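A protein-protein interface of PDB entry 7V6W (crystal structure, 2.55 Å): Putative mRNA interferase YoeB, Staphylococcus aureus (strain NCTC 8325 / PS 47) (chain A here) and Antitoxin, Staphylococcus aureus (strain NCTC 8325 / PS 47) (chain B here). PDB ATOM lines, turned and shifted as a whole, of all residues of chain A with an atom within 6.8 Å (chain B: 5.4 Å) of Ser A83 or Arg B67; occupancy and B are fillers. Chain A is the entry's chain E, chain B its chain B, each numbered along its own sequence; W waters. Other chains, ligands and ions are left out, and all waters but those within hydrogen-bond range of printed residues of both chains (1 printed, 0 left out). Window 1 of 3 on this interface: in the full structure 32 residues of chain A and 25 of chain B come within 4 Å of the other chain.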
ATOM      1  N   ILE A   9     -15.652 -18.534  16.599  1.00  0.00           N
ATOM      2  CA  ILE A   9     -16.778 -19.452  16.714  1.00  0.00           C
ATOM      3  C   ILE A   9     -17.602 -19.380  15.437  1.00  0.00           C
ATOM      4  O   ILE A   9     -17.771 -18.303  14.855  1.00  0.00           O
ATOM      5  CB  ILE A   9     -17.641 -19.134  17.957  1.00  0.00           C
ATOM      6  CG1 ILE A   9     -18.791 -20.136  18.095  1.00  0.00           C
ATOM      7  CG2 ILE A   9     -18.165 -17.704  17.907  1.00  0.00           C
ATOM      8  CD1 ILE A   9     -19.602 -19.964  19.359  1.00  0.00           C
ATOM      9  N   LYS A  10     -18.091 -20.534  14.985  1.00  0.00           N
ATOM     10  CA  LYS A  10     -19.021 -20.556  13.863  1.00  0.00           C
ATOM     11  C   LYS A  10     -20.268 -19.757  14.219  1.00  0.00           C
ATOM     12  O   LYS A  10     -20.800 -19.868  15.327  1.00  0.00           O
ATOM     13  CB  LYS A  10     -19.396 -21.996  13.504  1.00  0.00           C
ATOM     14  CG  LYS A  10     -18.719 -22.546  12.248  1.00  0.00           C
ATOM     15  CD  LYS A  10     -19.237 -21.865  10.986  1.00  0.00           C
ATOM     16  CE  LYS A  10     -18.983 -22.701   9.733  1.00  0.00           C
ATOM     17  NZ  LYS A  10     -17.545 -23.047   9.544  1.00  0.00           N
ATOM     18  N   SER A  12     -23.283 -20.038  13.249  1.00  0.00           N
ATOM     19  CA  SER A  12     -24.410 -20.902  13.577  1.00  0.00           C
ATOM     20  C   SER A  12     -24.309 -21.468  14.989  1.00  0.00           C
ATOM     21  O   SER A  12     -25.329 -21.884  15.549  1.00  0.00           O
ATOM     22  CB  SER A  12     -24.512 -22.037  12.557  1.00  0.00           C
ATOM     23  OG  SER A  12     -23.295 -22.756  12.467  1.00  0.00           O
ATOM     24  N   ALA A  13     -23.112 -21.487  15.573  1.00  0.00           N
ATOM     25  CA  ALA A  13     -22.914 -21.943  16.941  1.00  0.00           C
ATOM     26  C   ALA A  13     -23.072 -20.828  17.967  1.00  0.00           C
ATOM     27  O   ALA A  13     -22.955 -21.090  19.168  1.00  0.00           O
ATOM     28  CB  ALA A  13     -21.531 -22.585  17.092  1.00  0.00           C
ATOM     29  N   LYS A  14     -23.332 -19.592  17.526  1.00  0.00           N
ATOM     30  CA  LYS A  14     -23.556 -18.499  18.465  1.00  0.00           C
ATOM     31  C   LYS A  14     -24.844 -18.671  19.257  1.00  0.00           C
ATOM     32  O   LYS A  14     -25.006 -18.029  20.301  1.00  0.00           O
ATOM     33  CB  LYS A  14     -23.570 -17.161  17.721  1.00  0.00           C
ATOM     34  CG  LYS A  14     -22.252 -16.404  17.804  1.00  0.00           C
ATOM     35  CD  LYS A  14     -22.029 -15.517  16.587  1.00  0.00           C
ATOM     36  CE  LYS A  14     -23.147 -14.506  16.403  1.00  0.00           C
ATOM     37  NZ  LYS A  14     -22.900 -13.643  15.214  1.00  0.00           N
ATOM     38  N   SER A  15     -25.761 -19.521  18.787  1.00  0.00           N
ATOM     39  CA  SER A  15     -26.959 -19.823  19.563  1.00  0.00           C
ATOM     40  C   SER A  15     -26.606 -20.436  20.910  1.00  0.00           C
ATOM     41  O   SER A  15     -27.343 -20.258  21.887  1.00  0.00           O
ATOM     42  CB  SER A  15     -27.869 -20.767  18.778  1.00  0.00           C
ATOM     43  OG  SER A  15     -28.039 -20.318  17.444  1.00  0.00           O
ATOM     44  N   ASP A  16     -25.483 -21.158  20.981  1.00  0.00           N
ATOM     45  CA  ASP A  16     -25.065 -21.766  22.238  1.00  0.00           C
ATOM     46  C   ASP A  16     -24.647 -20.717  23.260  1.00  0.00           C
ATOM     47  O   ASP A  16     -24.856 -20.908  24.463  1.00  0.00           O
ATOM     48  CB  ASP A  16     -23.916 -22.744  21.990  1.00  0.00           C
ATOM     49  CG  ASP A  16     -24.301 -23.874  21.056  1.00  0.00           C
ATOM     50  OD1 ASP A  16     -25.498 -23.987  20.710  1.00  0.00           O
ATOM     51  OD2 ASP A  16     -23.403 -24.649  20.665  1.00  0.00           O
ATOM     52  N   LYS A  19     -27.492 -19.497  25.450  1.00  0.00           N
ATOM     53  CA  LYS A  19     -27.818 -20.432  26.522  1.00  0.00           C
ATOM     54  C   LYS A  19     -26.760 -20.416  27.616  1.00  0.00           C
ATOM     55  O   LYS A  19     -27.071 -20.681  28.783  1.00  0.00           O
ATOM     56  CB  LYS A  19     -27.977 -21.844  25.958  1.00  0.00           C
ATOM     57  CG  LYS A  19     -29.026 -21.963  24.867  1.00  0.00           C
ATOM     58  CD  LYS A  19     -29.055 -23.364  24.283  1.00  0.00           C
ATOM     59  CE  LYS A  19     -30.080 -23.474  23.168  1.00  0.00           C
ATOM     60  NZ  LYS A  19     -30.092 -24.832  22.558  1.00  0.00           N
ATOM     61  N   PHE A  29     -17.041 -20.142  30.655  1.00  0.00           N
ATOM     62  CA  PHE A  29     -16.749 -20.219  29.228  1.00  0.00           C
ATOM     63  C   PHE A  29     -15.574 -19.324  28.855  1.00  0.00           C
ATOM     64  O   PHE A  29     -14.698 -19.729  28.082  1.00  0.00           O
ATOM     65  CB  PHE A  29     -17.990 -19.843  28.418  1.00  0.00           C
ATOM     66  CG  PHE A  29     -17.747 -19.765  26.937  1.00  0.00           C
ATOM     67  CD1 PHE A  29     -17.672 -20.918  26.173  1.00  0.00           C
ATOM     68  CD2 PHE A  29     -17.599 -18.539  26.308  1.00  0.00           C
ATOM     69  CE1 PHE A  29     -17.449 -20.849  24.810  1.00  0.00           C
ATOM     70  CE2 PHE A  29     -17.375 -18.463  24.946  1.00  0.00           C
ATOM     71  CZ  PHE A  29     -17.300 -19.619  24.196  1.00  0.00           C
ATOM     72  N   ILE A  62     -16.888 -26.798  30.233  1.00  0.00           N
ATOM     73  CA  ILE A  62     -17.402 -25.619  30.921  1.00  0.00           C
ATOM     74  C   ILE A  62     -17.818 -25.985  32.339  1.00  0.00           C
ATOM     75  O   ILE A  62     -17.557 -25.239  33.290  1.00  0.00           O
ATOM     76  CB  ILE A  62     -18.566 -25.006  30.122  1.00  0.00           C
ATOM     77  CG1 ILE A  62     -18.127 -24.718  28.686  1.00  0.00           C
ATOM     78  CG2 ILE A  62     -19.063 -23.735  30.790  1.00  0.00           C
ATOM     79  CD1 ILE A  62     -19.231 -24.179  27.805  1.00  0.00           C
ATOM     80  N   ARG A  67     -19.694 -28.710  27.205  1.00  0.00           N
ATOM     81  CA  ARG A  67     -18.353 -28.767  26.653  1.00  0.00           C
ATOM     82  C   ARG A  67     -18.179 -27.678  25.605  1.00  0.00           C
ATOM     83  O   ARG A  67     -19.149 -27.156  25.050  1.00  0.00           O
ATOM     84  CB  ARG A  67     -18.060 -30.133  26.012  1.00  0.00           C
ATOM     85  CG  ARG A  67     -18.383 -31.329  26.890  1.00  0.00           C
ATOM     86  CD  ARG A  67     -17.488 -31.371  28.110  1.00  0.00           C
ATOM     87  NE  ARG A  67     -17.533 -32.673  28.769  1.00  0.00           N
ATOM     88  CZ  ARG A  67     -18.360 -32.982  29.761  1.00  0.00           C
ATOM     89  NH1 ARG A  67     -19.214 -32.079  30.222  1.00  0.00           N
ATOM     90  NH2 ARG A  67     -18.329 -34.195  30.295  1.00  0.00           N
ATOM     91  N   VAL A  68     -16.922 -27.346  25.340  1.00  0.00           N
ATOM     92  CA  VAL A  68     -16.543 -26.531  24.196  1.00  0.00           C
ATOM     93  C   VAL A  68     -15.864 -27.461  23.203  1.00  0.00           C
ATOM     94  O   VAL A  68     -14.754 -27.947  23.452  1.00  0.00           O
ATOM     95  CB  VAL A  68     -15.621 -25.369  24.587  1.00  0.00           C
ATOM     96  CG1 VAL A  68     -15.114 -24.661  23.339  1.00  0.00           C
ATOM     97  CG2 VAL A  68     -16.353 -24.393  25.490  1.00  0.00           C
ATOM     98  N   VAL A  69     -16.530 -27.728  22.090  1.00  0.00           N
ATOM     99  CA  VAL A  69     -15.966 -28.559  21.032  1.00  0.00           C
ATOM    100  C   VAL A  69     -15.339 -27.644  19.989  1.00  0.00           C
ATOM    101  O   VAL A  69     -15.963 -26.668  19.552  1.00  0.00           O
ATOM    102  CB  VAL A  69     -17.038 -29.467  20.408  1.00  0.00           C
ATOM    103  CG1 VAL A  69     -16.405 -30.422  19.413  1.00  0.00           C
ATOM    104  CG2 VAL A  69     -17.779 -30.234  21.497  1.00  0.00           C
ATOM    105  N   TYR A  70     -14.108 -27.951  19.593  1.00  0.00           N
ATOM    106  CA  TYR A  70     -13.377 -27.053  18.711  1.00  0.00           C
ATOM    107  C   TYR A  70     -12.325 -27.826  17.930  1.00  0.00           C
ATOM    108  O   TYR A  70     -11.928 -28.933  18.304  1.00  0.00           O
ATOM    109  CB  TYR A  70     -12.717 -25.914  19.500  1.00  0.00           C
ATOM    110  CG  TYR A  70     -11.681 -26.378  20.499  1.00  0.00           C
ATOM    111  CD1 TYR A  70     -12.053 -26.816  21.763  1.00  0.00           C
ATOM    112  CD2 TYR A  70     -10.331 -26.376  20.179  1.00  0.00           C
ATOM    113  CE1 TYR A  70     -11.109 -27.240  22.679  1.00  0.00           C
ATOM    114  CE2 TYR A  70      -9.380 -26.797  21.086  1.00  0.00           C
ATOM    115  CZ  TYR A  70      -9.774 -27.228  22.335  1.00  0.00           C
ATOM    116  OH  TYR A  70      -8.825 -27.647  23.241  1.00  0.00           O
ATOM    117  N   LEU A  80     -11.259 -22.794  16.238  1.00  0.00           N
ATOM    118  CA  LEU A  80     -12.619 -22.687  15.721  1.00  0.00           C
ATOM    119  C   LEU A  80     -13.561 -23.411  16.672  1.00  0.00           C
ATOM    120  O   LEU A  80     -13.591 -24.646  16.704  1.00  0.00           O
ATOM    121  CB  LEU A  80     -12.718 -23.267  14.311  1.00  0.00           C
ATOM    122  CG  LEU A  80     -14.126 -23.314  13.715  1.00  0.00           C
ATOM    123  CD1 LEU A  80     -14.758 -21.930  13.727  1.00  0.00           C
ATOM    124  CD2 LEU A  80     -14.097 -23.881  12.304  1.00  0.00           C
ATOM    125  N   ILE A  81     -14.330 -22.645  17.439  1.00  0.00           N
ATOM    126  CA  ILE A  81     -15.315 -23.219  18.346  1.00  0.00           C
ATOM    127  C   ILE A  81     -16.532 -23.642  17.535  1.00  0.00           C
ATOM    128  O   ILE A  81     -17.162 -22.818  16.863  1.00  0.00           O
ATOM    129  CB  ILE A  81     -15.704 -22.226  19.448  1.00  0.00           C
ATOM    130  CG1 ILE A  81     -14.518 -21.989  20.384  1.00  0.00           C
ATOM    131  CG2 ILE A  81     -16.916 -22.731  20.215  1.00  0.00           C
ATOM    132  CD1 ILE A  81     -14.811 -21.011  21.494  1.00  0.00           C
ATOM    133  N   LEU A  82     -16.864 -24.930  17.595  1.00  0.00           N
ATOM    134  CA  LEU A  82     -17.999 -25.477  16.865  1.00  0.00           C
ATOM    135  C   LEU A  82     -19.206 -25.747  17.750  1.00  0.00           C
ATOM    136  O   LEU A  82     -20.301 -25.967  17.224  1.00  0.00           O
ATOM    137  CB  LEU A  82     -17.589 -26.772  16.153  1.00  0.00           C
ATOM    138  CG  LEU A  82     -16.472 -26.625  15.118  1.00  0.00           C
ATOM    139  CD1 LEU A  82     -15.890 -27.983  14.762  1.00  0.00           C
ATOM    140  CD2 LEU A  82     -16.991 -25.918  13.877  1.00  0.00           C
ATOM    141  N   SER A  83     -19.040 -25.735  19.070  1.00  0.00           N
ATOM    142  CA  SER A  83     -20.151 -25.984  19.976  1.00  0.00           C
ATOM    143  C   SER A  83     -19.780 -25.488  21.364  1.00  0.00           C
ATOM    144  O   SER A  83     -18.634 -25.634  21.794  1.00  0.00           O
ATOM    145  CB  SER A  83     -20.508 -27.474  20.031  1.00  0.00           C
ATOM    146  OG  SER A  83     -21.604 -27.696  20.900  1.00  0.00           O
ATOM    147  N   ALA A  84     -20.755 -24.905  22.059  1.00  0.00           N
ATOM    148  CA  ALA A  84     -20.546 -24.492  23.441  1.00  0.00           C
ATOM    149  C   ALA A  84     -21.714 -24.901  24.331  1.00  0.00           C
ATOM    150  O   ALA A  84     -21.856 -24.364  25.435  1.00  0.00           O
ATOM    151  CB  ALA A  84     -20.307 -22.982  23.536  1.00  0.00           C
ATOM    152  N   TRP A  85     -22.545 -25.836  23.878  1.00  0.00           N
ATOM    153  CA  TRP A  85     -23.718 -26.273  24.627  1.00  0.00           C
ATOM    154  C   TRP A  85     -23.937 -27.746  24.325  1.00  0.00           C
ATOM    155  O   TRP A  85     -24.101 -28.119  23.160  1.00  0.00           O
ATOM    156  CB  TRP A  85     -24.948 -25.441  24.248  1.00  0.00           C
ATOM    157  CG  TRP A  85     -26.147 -25.694  25.106  1.00  0.00           C
ATOM    158  CD1 TRP A  85     -27.234 -26.456  24.792  1.00  0.00           C
ATOM    159  CD2 TRP A  85     -26.385 -25.177  26.421  1.00  0.00           C
ATOM    160  NE1 TRP A  85     -28.134 -26.446  25.829  1.00  0.00           N
ATOM    161  CE2 TRP A  85     -27.636 -25.669  26.842  1.00  0.00           C
ATOM    162  CE3 TRP A  85     -25.662 -24.349  27.284  1.00  0.00           C
ATOM    163  CZ2 TRP A  85     -28.180 -25.359  28.088  1.00  0.00           C
ATOM    164  CZ3 TRP A  85     -26.202 -24.043  28.521  1.00  0.00           C
ATOM    165  CH2 TRP A  85     -27.449 -24.547  28.910  1.00  0.00           C
ATOM    166  N   SER A  86     -23.933 -28.579  25.367  1.00  0.00           N
ATOM    167  CA  SER A  86     -23.932 -30.027  25.204  1.00  0.00           C
ATOM    168  C   SER A  86     -25.258 -30.669  25.600  1.00  0.00           C
ATOM    169  O   SER A  86     -25.308 -31.879  25.842  1.00  0.00           O
ATOM    170  CB  SER A  86     -22.786 -30.643  26.007  1.00  0.00           C
ATOM    171  OG  SER A  86     -21.546 -30.057  25.655  1.00  0.00           O
ATOM    172  N   THR B  60     -24.914 -33.539  20.310  1.00  0.00           N
ATOM    173  CA  THR B  60     -23.987 -32.429  20.118  1.00  0.00           C
ATOM    174  C   THR B  60     -23.106 -32.648  18.895  1.00  0.00           C
ATOM    175  O   THR B  60     -22.866 -31.713  18.123  1.00  0.00           O
ATOM    176  CB  THR B  60     -23.128 -32.242  21.369  1.00  0.00           C
ATOM    177  OG1 THR B  60     -23.976 -32.140  22.519  1.00  0.00           O
ATOM    178  CG2 THR B  60     -22.284 -30.980  21.255  1.00  0.00           C
ATOM    179  N   ASP B  62     -23.840 -34.257  16.244  1.00  0.00           N
ATOM    180  CA  ASP B  62     -24.641 -34.002  15.051  1.00  0.00           C
ATOM    181  C   ASP B  62     -24.677 -32.514  14.730  1.00  0.00           C
ATOM    182  O   ASP B  62     -24.643 -32.123  13.557  1.00  0.00           O
ATOM    183  CB  ASP B  62     -26.058 -34.544  15.233  1.00  0.00           C
ATOM    184  CG  ASP B  62     -26.097 -36.057  15.323  1.00  0.00           C
ATOM    185  OD1 ASP B  62     -25.175 -36.712  14.793  1.00  0.00           O
ATOM    186  OD2 ASP B  62     -27.055 -36.592  15.921  1.00  0.00           O
ATOM    187  N   LYS B  63     -24.747 -31.669  15.761  1.00  0.00           N
ATOM    188  CA  LYS B  63     -24.674 -30.230  15.538  1.00  0.00           C
ATOM    189  C   LYS B  63     -23.280 -29.817  15.088  1.00  0.00           C
ATOM    190  O   LYS B  63     -23.134 -28.959  14.209  1.00  0.00           O
ATOM    191  CB  LYS B  63     -25.076 -29.481  16.808  1.00  0.00           C
ATOM    192  CG  LYS B  63     -26.536 -29.653  17.196  1.00  0.00           C
ATOM    193  CD  LYS B  63     -26.905 -28.747  18.362  1.00  0.00           C
ATOM    194  CE  LYS B  63     -28.381 -28.867  18.720  1.00  0.00           C
ATOM    195  NZ  LYS B  63     -28.741 -30.233  19.201  1.00  0.00           N
ATOM    196  N   VAL B  64     -22.243 -30.425  15.668  1.00  0.00           N
ATOM    197  CA  VAL B  64     -20.871 -30.088  15.295  1.00  0.00           C
ATOM    198  C   VAL B  64     -20.614 -30.439  13.836  1.00  0.00           C
ATOM    199  O   VAL B  64     -20.056 -29.639  13.075  1.00  0.00           O
ATOM    200  CB  VAL B  64     -19.873 -30.795  16.230  1.00  0.00           C
ATOM    201  CG1 VAL B  64     -18.457 -30.660  15.697  1.00  0.00           C
ATOM    202  CG2 VAL B  64     -19.970 -30.224  17.634  1.00  0.00           C
ATOM    203  N   ARG B  65     -21.017 -31.645  13.422  1.00  0.00           N
ATOM    204  CA  ARG B  65     -20.799 -32.059  12.039  1.00  0.00           C
ATOM    205  C   ARG B  65     -21.602 -31.200  11.070  1.00  0.00           C
ATOM    206  O   ARG B  65     -21.119 -30.860   9.984  1.00  0.00           O
ATOM    207  CB  ARG B  65     -21.155 -33.536  11.868  1.00  0.00           C
ATOM    208  CG  ARG B  65     -20.115 -34.496  12.424  1.00  0.00           C
ATOM    209  CD  ARG B  65     -20.541 -35.941  12.223  1.00  0.00           C
ATOM    210  NE  ARG B  65     -21.655 -36.306  13.093  1.00  0.00           N
ATOM    211  CZ  ARG B  65     -21.514 -36.913  14.267  1.00  0.00           C
ATOM    212  NH1 ARG B  65     -20.306 -37.233  14.708  1.00  0.00           N
ATOM    213  NH2 ARG B  65     -22.581 -37.207  14.998  1.00  0.00           N
ATOM    214  N   GLU B  66     -22.830 -30.840  11.447  1.00  0.00           N
ATOM    215  CA  GLU B  66     -23.645 -29.988  10.589  1.00  0.00           C
ATOM    216  C   GLU B  66     -23.077 -28.577  10.517  1.00  0.00           C
ATOM    217  O   GLU B  66     -23.142 -27.926   9.468  1.00  0.00           O
ATOM    218  CB  GLU B  66     -25.087 -29.967  11.094  1.00  0.00           C
ATOM    219  CG  GLU B  66     -26.037 -29.141  10.247  1.00  0.00           C
ATOM    220  CD  GLU B  66     -27.461 -29.182  10.767  1.00  0.00           C
ATOM    221  OE1 GLU B  66     -27.682 -29.757  11.855  1.00  0.00           O
ATOM    222  OE2 GLU B  66     -28.357 -28.641  10.087  1.00  0.00           O
ATOM    223  N   ARG B  67     -22.506 -28.089  11.622  1.00  0.00           N
ATOM    224  CA  ARG B  67     -21.940 -26.746  11.625  1.00  0.00           C
ATOM    225  C   ARG B  67     -20.620 -26.686  10.864  1.00  0.00           C
ATOM    226  O   ARG B  67     -20.266 -25.631  10.327  1.00  0.00           O
ATOM    227  CB  ARG B  67     -21.751 -26.256  13.060  1.00  0.00           C
ATOM    228  CG  ARG B  67     -23.045 -25.860  13.751  1.00  0.00           C
ATOM    229  CD  ARG B  67     -22.820 -25.622  15.231  1.00  0.00           C
ATOM    230  NE  ARG B  67     -24.064 -25.322  15.929  1.00  0.00           N
ATOM    231  CZ  ARG B  67     -24.172 -25.228  17.250  1.00  0.00           C
ATOM    232  NH1 ARG B  67     -23.109 -25.416  18.020  1.00  0.00           N
ATOM    233  NH2 ARG B  67     -25.344 -24.949  17.803  1.00  0.00           N
ATOM    234  N   GLU B  68     -19.883 -27.796  10.807  1.00  0.00           N
ATOM    235  CA  GLU B  68     -18.641 -27.813  10.040  1.00  0.00           C
ATOM    236  C   GLU B  68     -18.895 -27.680   8.545  1.00  0.00           C
ATOM    237  O   GLU B  68     -18.019 -27.211   7.810  1.00  0.00           O
ATOM    238  CB  GLU B  68     -17.863 -29.097  10.318  1.00  0.00           C
ATOM    239  CG  GLU B  68     -16.977 -29.034  11.541  1.00  0.00           C
ATOM    240  CD  GLU B  68     -16.276 -30.350  11.818  1.00  0.00           C
ATOM    241  OE1 GLU B  68     -16.865 -31.412  11.522  1.00  0.00           O
ATOM    242  OE2 GLU B  68     -15.136 -30.321  12.325  1.00  0.00           O
ATOM    243  N   LYS B  69     -20.074 -28.084   8.076  1.00  0.00           N
ATOM    244  CA  LYS B  69     -20.364 -28.095   6.650  1.00  0.00           C
ATOM    245  C   LYS B  69     -21.123 -26.863   6.176  1.00  0.00           C
ATOM    246  O   LYS B  69     -21.258 -26.674   4.961  1.00  0.00           O
ATOM    247  CB  LYS B  69     -21.157 -29.355   6.284  1.00  0.00           C
ATOM    248  CG  LYS B  69     -20.331 -30.633   6.353  1.00  0.00           C
ATOM    249  CD  LYS B  69     -21.116 -31.855   5.897  1.00  0.00           C
ATOM    250  CE  LYS B  69     -22.161 -32.266   6.921  1.00  0.00           C
ATOM    251  NZ  LYS B  69     -22.819 -33.549   6.547  1.00  0.00           N
ATOM    252  N   ASP B  70     -21.614 -26.021   7.082  1.00  0.00           N
ATOM    253  CA  ASP B  70     -22.387 -24.870   6.651  1.00  0.00           C
ATOM    254  C   ASP B  70     -21.464 -23.711   6.285  1.00  0.00           C
ATOM    255  O   ASP B  70     -20.260 -23.728   6.547  1.00  0.00           O
ATOM    256  CB  ASP B  70     -23.378 -24.438   7.733  1.00  0.00           C
ATOM    257  CG  ASP B  70     -22.708 -23.712   8.887  1.00  0.00           C
ATOM    258  OD1 ASP B  70     -22.687 -24.267  10.000  1.00  0.00           O
ATOM    259  OD2 ASP B  70     -22.199 -22.591   8.686  1.00  0.00           O
HETATM  260  O   HOH W   1     -24.724 -27.347  20.357  1.00  0.00           O
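The side-chain hydroxyl of Ser A12 sits at hydrogen-bond distance from the side-chain carboxylate of Asp B70 (3.0 Å). The side-chain carboxylate of Asp A16 is in salt-bridge range of the guanidinium group of Arg B67 (2.8 Å). The backbone carbonyl oxygen (O) of Leu A82 lies within hydrogen-bond range of the guanidinium group (NH1) of Arg B67, at 3.0 Å.
The backbone NH (N) of Lys A10 is in hydrogen-bond range of the backbone carbonyl oxygen (O) of Ile A81, 3.1 Å away. The side-chain carboxylate (OD2) of Asp A16 sits at hydrogen-bond distance from the backbone NH (N) of Ala A84 (3.0 Å). The backbone NH (N) of Arg A67 lies within hydrogen-bond range of the side-chain hydroxyl (OG) of Ser A86. N of Leu A82 is in hydrogen-bond range of O of Val A69, at 2.8 Å. The backbone NH of Val A69 lies within hydrogen-bond range of the backbone carbonyl oxygen of Ser A83, 3.0 Å away. The side-chain hydroxyl (OG) of Ser A83 sits at hydrogen-bond distance from the backbone carbonyl oxygen (O) of Trp A85.
Lys A10 touches Arg B67. CE of Lys A10 touches OD2 of Asp B70, at 3.4 Å. OG of Ser A12 touches CG of Arg B67, 3.4 Å away. Arg B67 touches Ala A13. Val A69 touches Val B64 (CG1 to CG2, 3.99 Å). Val B64 touches Leu A82 (CG1 to CD1, 3.8 Å). Thr B60 touches Ser A83 (CG2 to OG, 3.4 Å). Val B64 touches Ser A83 (CG2 to CB, 3.7 Å). CA of Ser A83 touches NH1 of Arg B67 (3.6 Å). Thr B60 touches Trp A85.
Printed residues of chain B within 4 Å of Lys A10: Arg B67 and Asp B70. Of the printed residues of chain B, Val A69 touches Val B64. Ser A83 touches three residues of chain B. Asp B62 touches none of the printed residues of chain A. Arg B67 touches six residues of chain A. The nearest printed residue of chain B that does not touch Ser A83 is Lys B63 (5.7 Å). The nearest printed residue of chain B that does not touch Trp A85 is Lys B63 (5.6 Å).
Of the 21 printed residues of chain A, 9 touch a printed residue of chain B. Printed residues of chain A that touch a printed residue of chain B: Lys A10, Ser A12, Ala A13, Asp A16, Val A69, Leu A82, Ser A83, Trp A85 and Ser A86. Hydrophobic or aromatic side chains of chain A that line the printed part of chain B: Ala A13, Val A69 and Leu A82. Printed residues of chain B that touch a printed residue of chain A: Thr B60, Val B64, Arg B67, Glu B68 and Asp B70. Along chain B the printed residues that touch a printed residue of chain A span positions 60 to 70. Among the printed residues, 15 pairs touch across the chains. Among the printed residues, Asp or Glu carboxylates within 4 Å of a Lys or Arg side-chain nitrogen of the other chain: Asp A16 with Arg B67.
Water W1 lies within hydrogen-bond range of O of Trp A85 (3.0 Å), OD2 of Asp A16 (3.0 Å), OG of Ser A83 (3.2 Å) and NH1 of Arg B67 (3.4 Å).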
